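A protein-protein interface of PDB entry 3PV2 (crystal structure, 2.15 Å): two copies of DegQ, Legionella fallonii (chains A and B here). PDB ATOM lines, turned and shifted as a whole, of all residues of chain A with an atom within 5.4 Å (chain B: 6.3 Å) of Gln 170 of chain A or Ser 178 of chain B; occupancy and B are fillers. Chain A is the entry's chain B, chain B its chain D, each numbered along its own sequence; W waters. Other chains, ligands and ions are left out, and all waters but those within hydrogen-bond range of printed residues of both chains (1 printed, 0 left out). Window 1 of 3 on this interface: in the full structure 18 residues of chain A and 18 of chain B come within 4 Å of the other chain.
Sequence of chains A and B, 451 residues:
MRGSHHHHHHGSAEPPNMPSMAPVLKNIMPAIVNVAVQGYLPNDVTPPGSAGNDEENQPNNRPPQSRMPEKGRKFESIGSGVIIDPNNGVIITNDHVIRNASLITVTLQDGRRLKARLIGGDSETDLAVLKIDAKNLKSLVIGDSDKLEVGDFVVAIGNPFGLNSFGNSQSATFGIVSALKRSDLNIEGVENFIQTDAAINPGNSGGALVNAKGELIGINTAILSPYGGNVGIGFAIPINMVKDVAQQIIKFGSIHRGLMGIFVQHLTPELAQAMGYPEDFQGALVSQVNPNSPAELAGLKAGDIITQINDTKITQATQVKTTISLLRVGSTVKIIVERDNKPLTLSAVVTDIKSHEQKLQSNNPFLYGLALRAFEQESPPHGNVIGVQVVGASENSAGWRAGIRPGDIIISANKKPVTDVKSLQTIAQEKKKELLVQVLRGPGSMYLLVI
The backbone carbonyl oxygen (O) of Ala 172 of chain A sits at hydrogen-bond distance from the side-chain hydroxyl (OG) of Ser 178 of chain B, at 2.8 Å.
The side-chain hydroxyl (OG1) of Thr 196 of chain B lies within hydrogen-bond range of the backbone carbonyl oxygen (O) of Ile 176 of chain B (2.6 Å). The backbone NH (N) of Ile 176 of chain B sits at hydrogen-bond distance from the side-chain carboxylate (OD1) of Asp 197 of chain B. The backbone carbonyl oxygen of Ser 171 of chain A lies within hydrogen-bond range of the backbone NH of Gly 158 of chain A, at 2.9 Å. The side-chain hydroxyl (OG) of Ser 178 of chain B is in hydrogen-bond range of the backbone NH (N) of Asp 197 of chain B. The backbone NH of Gln 195 of chain B is in hydrogen-bond range of the backbone carbonyl oxygen of Ala 179 of chain B (2.8 Å). The backbone carbonyl oxygen (O) of Gln 195 of chain B is in hydrogen-bond range of the backbone NH (N) of Ser 178 of chain B.
Asn 168 of chain A touches Leu 180 of chain B (CB to O, 3.0 Å). Gln 170 of chain A touches Ser 178 of chain B (O to O, 3.6 Å). Gln 170 of chain A touches Ala 179 of chain B (O to CB, 3.3 Å). Ser 178 of chain B touches Ser 171 of chain A (O to CA, 3.3 Å). Gln 195 of chain B touches Ser 171 of chain A. Ala 172 of chain A touches Val 150 of chain B. Ala 172 of chain A touches Ile 176 of chain B (O to CD1, 3.6 Å). CD1 of Ile 176 of chain B touches C of Thr 173 of chain A, at 3.9 Å. CA of Thr 173 of chain A touches OD2 of Asp 197 of chain B (3.5 Å).
Of the printed residues of chain B, Asn 168 of chain A touches Leu 180 (3.0 Å). Ser 169 of chain A touches none of the printed residues of chain B. Gln 170 of chain A touches just these residues of chain B: Ser 178 (3.6 Å) and Ala 179 (3.3 Å). Of the printed residues of chain A, Leu 180 of chain B touches Asn 168 (3.0 Å). Of the printed residues of chain A, Gln 195 of chain B touches Ser 171. Ala 198 of chain B touches none of the printed residues of chain A.
Printed residues of chain B that touch a printed residue of chain A: Val 150, Ile 176, Ser 178, Ala 179, Leu 180, Gln 195 and Asp 197. Hydrophobic or aromatic side chains of chain B within 4 Å of the printed part of chain A: Val 150, Ile 176, Ala 179 and Leu 180. Hydrophobic or aromatic side chains of chain A within 4 Å of the printed part of chain B: Ala 172. Along chain A the printed residues that touch a printed residue of chain B span positions 168 to 173. Among the printed residues, 10 pairs touch across the chains. Among the printed residues, no Asp or Glu carboxylate lies within 4 Å of a Lys or Arg side-chain nitrogen of the other chain.
No position is printed for both chains. Of the 10 pairs that touch across the chains among the printed residues, none has its exchanged pair printed and touching as well.
Water W1 lies within hydrogen-bond range of the backbone carbonyl oxygen (O) of Asn 168 of chain A (2.8 Å), the backbone carbonyl oxygen (O) of Gln 170 of chain A (3.0 Å) and the backbone NH (N) of Leu 180 of chain B (3.1 Å).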
ATOM      1  N   MET A  29     -21.477 -37.568 -17.574  1.00  0.00           N
ATOM      2  CA  MET A  29     -21.565 -36.144 -17.226  1.00  0.00           C
ATOM      3  C   MET A  29     -22.206 -35.842 -15.875  1.00  0.00           C
ATOM      4  O   MET A  29     -21.749 -34.964 -15.188  1.00  0.00           O
ATOM      5  CB  MET A  29     -22.356 -35.368 -18.283  1.00  0.00           C
ATOM      6  CG  MET A  29     -21.589 -34.983 -19.532  1.00  0.00           C
ATOM      7  SD  MET A  29     -22.726 -34.015 -20.630  1.00  0.00           S
ATOM      8  CE  MET A  29     -22.134 -34.432 -22.305  1.00  0.00           C
ATOM      9  N   PRO A  30     -23.279 -36.545 -15.489  1.00  0.00           N
ATOM     10  CA  PRO A  30     -23.775 -36.190 -14.146  1.00  0.00           C
ATOM     11  C   PRO A  30     -22.779 -36.414 -12.987  1.00  0.00           C
ATOM     12  O   PRO A  30     -23.034 -35.961 -11.876  1.00  0.00           O
ATOM     13  CB  PRO A  30     -25.009 -37.043 -13.970  1.00  0.00           C
ATOM     14  CG  PRO A  30     -25.395 -37.501 -15.380  1.00  0.00           C
ATOM     15  CD  PRO A  30     -24.160 -37.489 -16.201  1.00  0.00           C
ATOM     16  N   ILE A  32     -19.685 -35.280 -12.967  1.00  0.00           N
ATOM     17  CA  ILE A  32     -18.681 -34.221 -13.022  1.00  0.00           C
ATOM     18  C   ILE A  32     -19.308 -32.927 -12.504  1.00  0.00           C
ATOM     19  O   ILE A  32     -20.344 -32.499 -13.010  1.00  0.00           O
ATOM     20  CB  ILE A  32     -18.287 -33.924 -14.421  1.00  0.00           C
ATOM     21  CG1 ILE A  32     -17.948 -35.231 -15.179  1.00  0.00           C
ATOM     22  CG2 ILE A  32     -17.038 -32.960 -14.462  1.00  0.00           C
ATOM     23  CD1 ILE A  32     -16.950 -36.122 -14.507  1.00  0.00           C
ATOM     24  N   GLN A 109     -24.742 -30.997 -12.347  1.00  0.00           N
ATOM     25  CA  GLN A 109     -25.240 -30.761 -13.656  1.00  0.00           C
ATOM     26  C   GLN A 109     -26.721 -30.419 -13.607  1.00  0.00           C
ATOM     27  O   GLN A 109     -27.153 -29.539 -14.305  1.00  0.00           O
ATOM     28  CB  GLN A 109     -25.015 -32.009 -14.462  1.00  0.00           C
ATOM     29  CG  GLN A 109     -25.546 -31.958 -15.828  1.00  0.00           C
ATOM     30  CD  GLN A 109     -25.943 -33.324 -16.280  1.00  0.00           C
ATOM     31  OE1 GLN A 109     -25.311 -33.908 -17.173  1.00  0.00           O
ATOM     32  NE2 GLN A 109     -26.985 -33.870 -15.639  1.00  0.00           N
ATOM     33  N   ILE A 157     -12.771 -34.252 -19.036  1.00  0.00           N
ATOM     34  CA  ILE A 157     -14.031 -33.587 -18.847  1.00  0.00           C
ATOM     35  C   ILE A 157     -14.010 -32.761 -17.568  1.00  0.00           C
ATOM     36  O   ILE A 157     -13.686 -33.284 -16.476  1.00  0.00           O
ATOM     37  CB  ILE A 157     -15.188 -34.563 -18.608  1.00  0.00           C
ATOM     38  CG1 ILE A 157     -15.077 -35.782 -19.491  1.00  0.00           C
ATOM     39  CG2 ILE A 157     -16.564 -33.841 -18.886  1.00  0.00           C
ATOM     40  CD1 ILE A 157     -16.172 -36.826 -19.114  1.00  0.00           C
ATOM     41  N   GLY A 158     -14.435 -31.504 -17.658  1.00  0.00           N
ATOM     42  CA  GLY A 158     -14.677 -30.749 -16.434  1.00  0.00           C
ATOM     43  C   GLY A 158     -16.035 -30.107 -16.473  1.00  0.00           C
ATOM     44  O   GLY A 158     -16.809 -30.296 -17.407  1.00  0.00           O
ATOM     45  N   ASN A 159     -16.317 -29.326 -15.454  1.00  0.00           N
ATOM     46  CA  ASN A 159     -17.562 -28.586 -15.434  1.00  0.00           C
ATOM     47  C   ASN A 159     -17.121 -27.266 -14.921  1.00  0.00           C
ATOM     48  O   ASN A 159     -17.275 -26.981 -13.724  1.00  0.00           O
ATOM     49  CB  ASN A 159     -18.588 -29.253 -14.541  1.00  0.00           C
ATOM     50  CG  ASN A 159     -19.927 -28.456 -14.413  1.00  0.00           C
ATOM     51  OD1 ASN A 159     -20.050 -27.264 -14.740  1.00  0.00           O
ATOM     52  ND2 ASN A 159     -20.925 -29.141 -13.888  1.00  0.00           N
ATOM     53  N   PRO A 160     -16.493 -26.469 -15.804  1.00  0.00           N
ATOM     54  CA  PRO A 160     -15.935 -25.245 -15.300  1.00  0.00           C
ATOM     55  C   PRO A 160     -16.958 -24.155 -15.099  1.00  0.00           C
ATOM     56  O   PRO A 160     -16.658 -23.211 -14.406  1.00  0.00           O
ATOM     57  CB  PRO A 160     -14.976 -24.829 -16.401  1.00  0.00           C
ATOM     58  CG  PRO A 160     -15.649 -25.286 -17.630  1.00  0.00           C
ATOM     59  CD  PRO A 160     -16.340 -26.570 -17.260  1.00  0.00           C
ATOM     60  N   PHE A 161     -18.143 -24.266 -15.686  1.00  0.00           N
ATOM     61  CA  PHE A 161     -19.032 -23.102 -15.718  1.00  0.00           C
ATOM     62  C   PHE A 161     -20.166 -23.084 -14.686  1.00  0.00           C
ATOM     63  O   PHE A 161     -20.567 -22.004 -14.263  1.00  0.00           O
ATOM     64  CB  PHE A 161     -19.620 -22.910 -17.117  1.00  0.00           C
ATOM     65  CG  PHE A 161     -18.586 -22.745 -18.204  1.00  0.00           C
ATOM     66  CD1 PHE A 161     -17.717 -21.658 -18.201  1.00  0.00           C
ATOM     67  CD2 PHE A 161     -18.516 -23.668 -19.257  1.00  0.00           C
ATOM     68  CE1 PHE A 161     -16.783 -21.501 -19.221  1.00  0.00           C
ATOM     69  CE2 PHE A 161     -17.586 -23.531 -20.279  1.00  0.00           C
ATOM     70  CZ  PHE A 161     -16.711 -22.454 -20.267  1.00  0.00           C
ATOM     71  N   ASN A 168     -25.457 -26.963 -20.524  1.00  0.00           N
ATOM     72  CA  ASN A 168     -24.223 -26.921 -21.306  1.00  0.00           C
ATOM     73  C   ASN A 168     -23.058 -26.369 -20.474  1.00  0.00           C
ATOM     74  O   ASN A 168     -22.286 -25.547 -20.938  1.00  0.00           O
ATOM     75  CB  ASN A 168     -24.399 -26.072 -22.561  1.00  0.00           C
ATOM     76  CG  ASN A 168     -25.585 -26.480 -23.383  1.00  0.00           C
ATOM     77  OD1 ASN A 168     -26.543 -25.736 -23.484  1.00  0.00           O
ATOM     78  ND2 ASN A 168     -25.534 -27.660 -23.975  1.00  0.00           N
ATOM     79  N   SER A 169     -22.958 -26.789 -19.223  1.00  0.00           N
ATOM     80  CA  SER A 169     -21.913 -26.263 -18.362  1.00  0.00           C
ATOM     81  C   SER A 169     -20.643 -27.090 -18.441  1.00  0.00           C
ATOM     82  O   SER A 169     -19.641 -26.728 -17.857  1.00  0.00           O
ATOM     83  CB  SER A 169     -22.394 -26.172 -16.919  1.00  0.00           C
ATOM     84  OG  SER A 169     -22.955 -27.404 -16.504  1.00  0.00           O
ATOM     85  N   GLN A 170     -20.670 -28.197 -19.157  1.00  0.00           N
ATOM     86  CA  GLN A 170     -19.475 -29.031 -19.200  1.00  0.00           C
ATOM     87  C   GLN A 170     -18.558 -28.728 -20.382  1.00  0.00           C
ATOM     88  O   GLN A 170     -18.938 -28.075 -21.371  1.00  0.00           O
ATOM     89  CB  GLN A 170     -19.858 -30.477 -19.150  1.00  0.00           C
ATOM     90  CG  GLN A 170     -20.950 -30.612 -18.079  1.00  0.00           C
ATOM     91  CD  GLN A 170     -20.926 -31.906 -17.335  1.00  0.00           C
ATOM     92  OE1 GLN A 170     -21.486 -32.012 -16.226  1.00  0.00           O
ATOM     93  NE2 GLN A 170     -20.313 -32.932 -17.954  1.00  0.00           N
ATOM     94  N   SER A 171     -17.344 -29.212 -20.241  1.00  0.00           N
ATOM     95  CA  SER A 171     -16.285 -28.932 -21.196  1.00  0.00           C
ATOM     96  C   SER A 171     -15.532 -30.219 -21.375  1.00  0.00           C
ATOM     97  O   SER A 171     -15.097 -30.785 -20.399  1.00  0.00           O
ATOM     98  CB  SER A 171     -15.396 -27.849 -20.596  1.00  0.00           C
ATOM     99  OG  SER A 171     -14.432 -27.350 -21.498  1.00  0.00           O
ATOM    100  N   ALA A 172     -15.355 -30.671 -22.605  1.00  0.00           N
ATOM    101  CA  ALA A 172     -14.621 -31.918 -22.902  1.00  0.00           C
ATOM    102  C   ALA A 172     -13.525 -31.717 -23.971  1.00  0.00           C
ATOM    103  O   ALA A 172     -13.747 -31.033 -24.899  1.00  0.00           O
ATOM    104  CB  ALA A 172     -15.605 -33.002 -23.355  1.00  0.00           C
ATOM    105  N   THR A 173     -12.369 -32.358 -23.831  1.00  0.00           N
ATOM    106  CA  THR A 173     -11.310 -32.339 -24.807  1.00  0.00           C
ATOM    107  C   THR A 173     -10.841 -33.777 -25.051  1.00  0.00           C
ATOM    108  O   THR A 173     -10.994 -34.639 -24.193  1.00  0.00           O
ATOM    109  CB  THR A 173     -10.139 -31.457 -24.319  1.00  0.00           C
ATOM    110  OG1 THR A 173      -9.671 -31.967 -23.056  1.00  0.00           O
ATOM    111  CG2 THR A 173     -10.616 -29.996 -24.127  1.00  0.00           C
ATOM    112  N   GLU B 149     -23.691 -32.590 -30.215  1.00  0.00           N
ATOM    113  CA  GLU B 149     -23.395 -32.833 -28.833  1.00  0.00           C
ATOM    114  C   GLU B 149     -21.894 -32.853 -28.537  1.00  0.00           C
ATOM    115  O   GLU B 149     -21.079 -33.181 -29.414  1.00  0.00           O
ATOM    116  CB  GLU B 149     -23.976 -34.184 -28.423  1.00  0.00           C
ATOM    117  CG  GLU B 149     -25.278 -34.594 -29.142  1.00  0.00           C
ATOM    118  CD  GLU B 149     -25.943 -35.774 -28.441  1.00  0.00           C
ATOM    119  OE1 GLU B 149     -25.765 -36.932 -28.892  1.00  0.00           O
ATOM    120  OE2 GLU B 149     -26.608 -35.538 -27.412  1.00  0.00           O
ATOM    121  N   VAL B 150     -21.586 -32.540 -27.280  1.00  0.00           N
ATOM    122  CA  VAL B 150     -20.261 -32.596 -26.704  1.00  0.00           C
ATOM    123  C   VAL B 150     -19.724 -34.006 -26.891  1.00  0.00           C
ATOM    124  O   VAL B 150     -20.430 -34.976 -26.624  1.00  0.00           O
ATOM    125  CB  VAL B 150     -20.300 -32.254 -25.247  1.00  0.00           C
ATOM    126  CG1 VAL B 150     -19.024 -32.735 -24.552  1.00  0.00           C
ATOM    127  CG2 VAL B 150     -20.498 -30.758 -25.110  1.00  0.00           C
ATOM    128  N   GLY B 151     -18.550 -34.107 -27.508  1.00  0.00           N
ATOM    129  CA  GLY B 151     -18.042 -35.410 -27.945  1.00  0.00           C
ATOM    130  C   GLY B 151     -18.045 -35.713 -29.424  1.00  0.00           C
ATOM    131  O   GLY B 151     -17.354 -36.647 -29.856  1.00  0.00           O
ATOM    132  N   ASP B 152     -18.841 -35.000 -30.222  1.00  0.00           N
ATOM    133  CA  ASP B 152     -18.886 -35.299 -31.628  1.00  0.00           C
ATOM    134  C   ASP B 152     -17.539 -34.913 -32.225  1.00  0.00           C
ATOM    135  O   ASP B 152     -16.948 -33.946 -31.792  1.00  0.00           O
ATOM    136  CB  ASP B 152     -19.981 -34.489 -32.325  1.00  0.00           C
ATOM    137  CG  ASP B 152     -21.416 -35.015 -32.045  1.00  0.00           C
ATOM    138  OD1 ASP B 152     -21.547 -36.188 -31.640  1.00  0.00           O
ATOM    139  OD2 ASP B 152     -22.419 -34.266 -32.277  1.00  0.00           O
ATOM    140  N   ILE B 176     -12.957 -32.425 -31.122  1.00  0.00           N
ATOM    141  CA  ILE B 176     -14.347 -32.665 -30.801  1.00  0.00           C
ATOM    142  C   ILE B 176     -15.080 -31.409 -30.444  1.00  0.00           C
ATOM    143  O   ILE B 176     -14.468 -30.384 -30.242  1.00  0.00           O
ATOM    144  CB  ILE B 176     -14.524 -33.630 -29.597  1.00  0.00           C
ATOM    145  CG1 ILE B 176     -13.870 -33.091 -28.345  1.00  0.00           C
ATOM    146  CG2 ILE B 176     -13.896 -34.956 -29.928  1.00  0.00           C
ATOM    147  CD1 ILE B 176     -14.153 -33.924 -27.024  1.00  0.00           C
ATOM    148  N   VAL B 177     -16.414 -31.500 -30.363  1.00  0.00           N
ATOM    149  CA  VAL B 177     -17.200 -30.443 -29.801  1.00  0.00           C
ATOM    150  C   VAL B 177     -16.937 -30.539 -28.309  1.00  0.00           C
ATOM    151  O   VAL B 177     -17.178 -31.599 -27.696  1.00  0.00           O
ATOM    152  CB  VAL B 177     -18.666 -30.637 -30.058  1.00  0.00           C
ATOM    153  CG1 VAL B 177     -19.542 -29.582 -29.254  1.00  0.00           C
ATOM    154  CG2 VAL B 177     -18.926 -30.601 -31.488  1.00  0.00           C
ATOM    155  N   SER B 178     -16.410 -29.451 -27.753  1.00  0.00           N
ATOM    156  CA  SER B 178     -16.032 -29.359 -26.363  1.00  0.00           C
ATOM    157  C   SER B 178     -17.161 -28.865 -25.490  1.00  0.00           C
ATOM    158  O   SER B 178     -17.289 -29.312 -24.344  1.00  0.00           O
ATOM    159  CB  SER B 178     -14.833 -28.416 -26.170  1.00  0.00           C
ATOM    160  OG  SER B 178     -13.690 -28.983 -26.761  1.00  0.00           O
ATOM    161  N   ALA B 179     -17.955 -27.936 -26.008  1.00  0.00           N
ATOM    162  CA  ALA B 179     -19.022 -27.305 -25.217  1.00  0.00           C
ATOM    163  C   ALA B 179     -19.902 -26.566 -26.173  1.00  0.00           C
ATOM    164  O   ALA B 179     -19.455 -26.136 -27.237  1.00  0.00           O
ATOM    165  CB  ALA B 179     -18.449 -26.330 -24.144  1.00  0.00           C
ATOM    166  N   LEU B 180     -21.180 -26.459 -25.812  1.00  0.00           N
ATOM    167  CA  LEU B 180     -22.149 -25.710 -26.599  1.00  0.00           C
ATOM    168  C   LEU B 180     -22.645 -24.597 -25.713  1.00  0.00           C
ATOM    169  O   LEU B 180     -22.490 -24.676 -24.481  1.00  0.00           O
ATOM    170  CB  LEU B 180     -23.290 -26.608 -26.976  1.00  0.00           C
ATOM    171  CG  LEU B 180     -22.931 -27.819 -27.816  1.00  0.00           C
ATOM    172  CD1 LEU B 180     -24.037 -28.884 -27.730  1.00  0.00           C
ATOM    173  CD2 LEU B 180     -22.688 -27.375 -29.253  1.00  0.00           C
ATOM    174  N   ILE B 194     -20.272 -22.641 -30.532  1.00  0.00           N
ATOM    175  CA  ILE B 194     -19.756 -23.961 -30.364  1.00  0.00           C
ATOM    176  C   ILE B 194     -18.298 -23.834 -29.944  1.00  0.00           C
ATOM    177  O   ILE B 194     -17.503 -23.107 -30.580  1.00  0.00           O
ATOM    178  CB  ILE B 194     -19.817 -24.714 -31.681  1.00  0.00           C
ATOM    179  CG1 ILE B 194     -21.265 -24.932 -32.132  1.00  0.00           C
ATOM    180  CG2 ILE B 194     -19.114 -26.051 -31.554  1.00  0.00           C
ATOM    181  CD1 ILE B 194     -21.372 -25.183 -33.660  1.00  0.00           C
ATOM    182  N   GLN B 195     -17.906 -24.539 -28.906  1.00  0.00           N
ATOM    183  CA  GLN B 195     -16.483 -24.566 -28.570  1.00  0.00           C
ATOM    184  C   GLN B 195     -15.904 -25.915 -29.009  1.00  0.00           C
ATOM    185  O   GLN B 195     -16.608 -26.952 -28.853  1.00  0.00           O
ATOM    186  CB  GLN B 195     -16.312 -24.343 -27.111  1.00  0.00           C
ATOM    187  CG  GLN B 195     -14.877 -24.322 -26.588  1.00  0.00           C
ATOM    188  CD  GLN B 195     -14.866 -24.216 -25.023  1.00  0.00           C
ATOM    189  OE1 GLN B 195     -15.540 -23.348 -24.444  1.00  0.00           O
ATOM    190  NE2 GLN B 195     -14.093 -25.111 -24.357  1.00  0.00           N
ATOM    191  N   THR B 196     -14.677 -25.896 -29.506  1.00  0.00           N
ATOM    192  CA  THR B 196     -14.006 -27.132 -30.003  1.00  0.00           C
ATOM    193  C   THR B 196     -12.560 -27.181 -29.619  1.00  0.00           C
ATOM    194  O   THR B 196     -12.009 -26.161 -29.307  1.00  0.00           O
ATOM    195  CB  THR B 196     -14.125 -27.225 -31.554  1.00  0.00           C
ATOM    196  OG1 THR B 196     -13.759 -28.553 -31.966  1.00  0.00           O
ATOM    197  CG2 THR B 196     -13.230 -26.310 -32.209  1.00  0.00           C
ATOM    198  N   ASP B 197     -11.921 -28.338 -29.566  1.00  0.00           N
ATOM    199  CA  ASP B 197     -10.484 -28.341 -29.449  1.00  0.00           C
ATOM    200  C   ASP B 197      -9.760 -28.589 -30.807  1.00  0.00           C
ATOM    201  O   ASP B 197      -8.618 -28.873 -30.805  1.00  0.00           O
ATOM    202  CB  ASP B 197      -9.968 -29.298 -28.367  1.00  0.00           C
ATOM    203  CG  ASP B 197     -10.336 -30.761 -28.614  1.00  0.00           C
ATOM    204  OD1 ASP B 197     -11.132 -30.986 -29.528  1.00  0.00           O
ATOM    205  OD2 ASP B 197      -9.822 -31.682 -27.900  1.00  0.00           O
ATOM    206  N   ALA B 198     -10.453 -28.478 -31.935  1.00  0.00           N
ATOM    207  CA  ALA B 198      -9.851 -28.450 -33.237  1.00  0.00           C
ATOM    208  C   ALA B 198      -9.328 -26.999 -33.357  1.00  0.00           C
ATOM    209  O   ALA B 198     -10.096 -26.044 -33.393  1.00  0.00           O
ATOM    210  CB  ALA B 198     -10.890 -28.744 -34.325  1.00  0.00           C
ATOM    211  N   GLY B 232      -6.109 -24.984 -27.516  1.00  0.00           N
ATOM    212  CA  GLY B 232      -7.050 -26.142 -27.489  1.00  0.00           C
ATOM    213  C   GLY B 232      -8.455 -25.700 -27.059  1.00  0.00           C
ATOM    214  O   GLY B 232      -9.170 -26.422 -26.328  1.00  0.00           O
ATOM    215  N   ILE B 233      -8.805 -24.478 -27.479  1.00  0.00           N
ATOM    216  CA  ILE B 233     -10.093 -23.861 -27.264  1.00  0.00           C
ATOM    217  C   ILE B 233     -10.299 -23.001 -28.477  1.00  0.00           C
ATOM    218  O   ILE B 233      -9.774 -21.900 -28.520  1.00  0.00           O
ATOM    219  CB  ILE B 233     -10.100 -22.879 -26.098  1.00  0.00           C
ATOM    220  CG1 ILE B 233      -9.840 -23.559 -24.772  1.00  0.00           C
ATOM    221  CG2 ILE B 233     -11.449 -22.159 -25.994  1.00  0.00           C
ATOM    222  CD1 ILE B 233      -9.437 -22.547 -23.678  1.00  0.00           C
HETATM  223  O   HOH W   1     -21.431 -27.377 -22.862  1.00  0.00           O
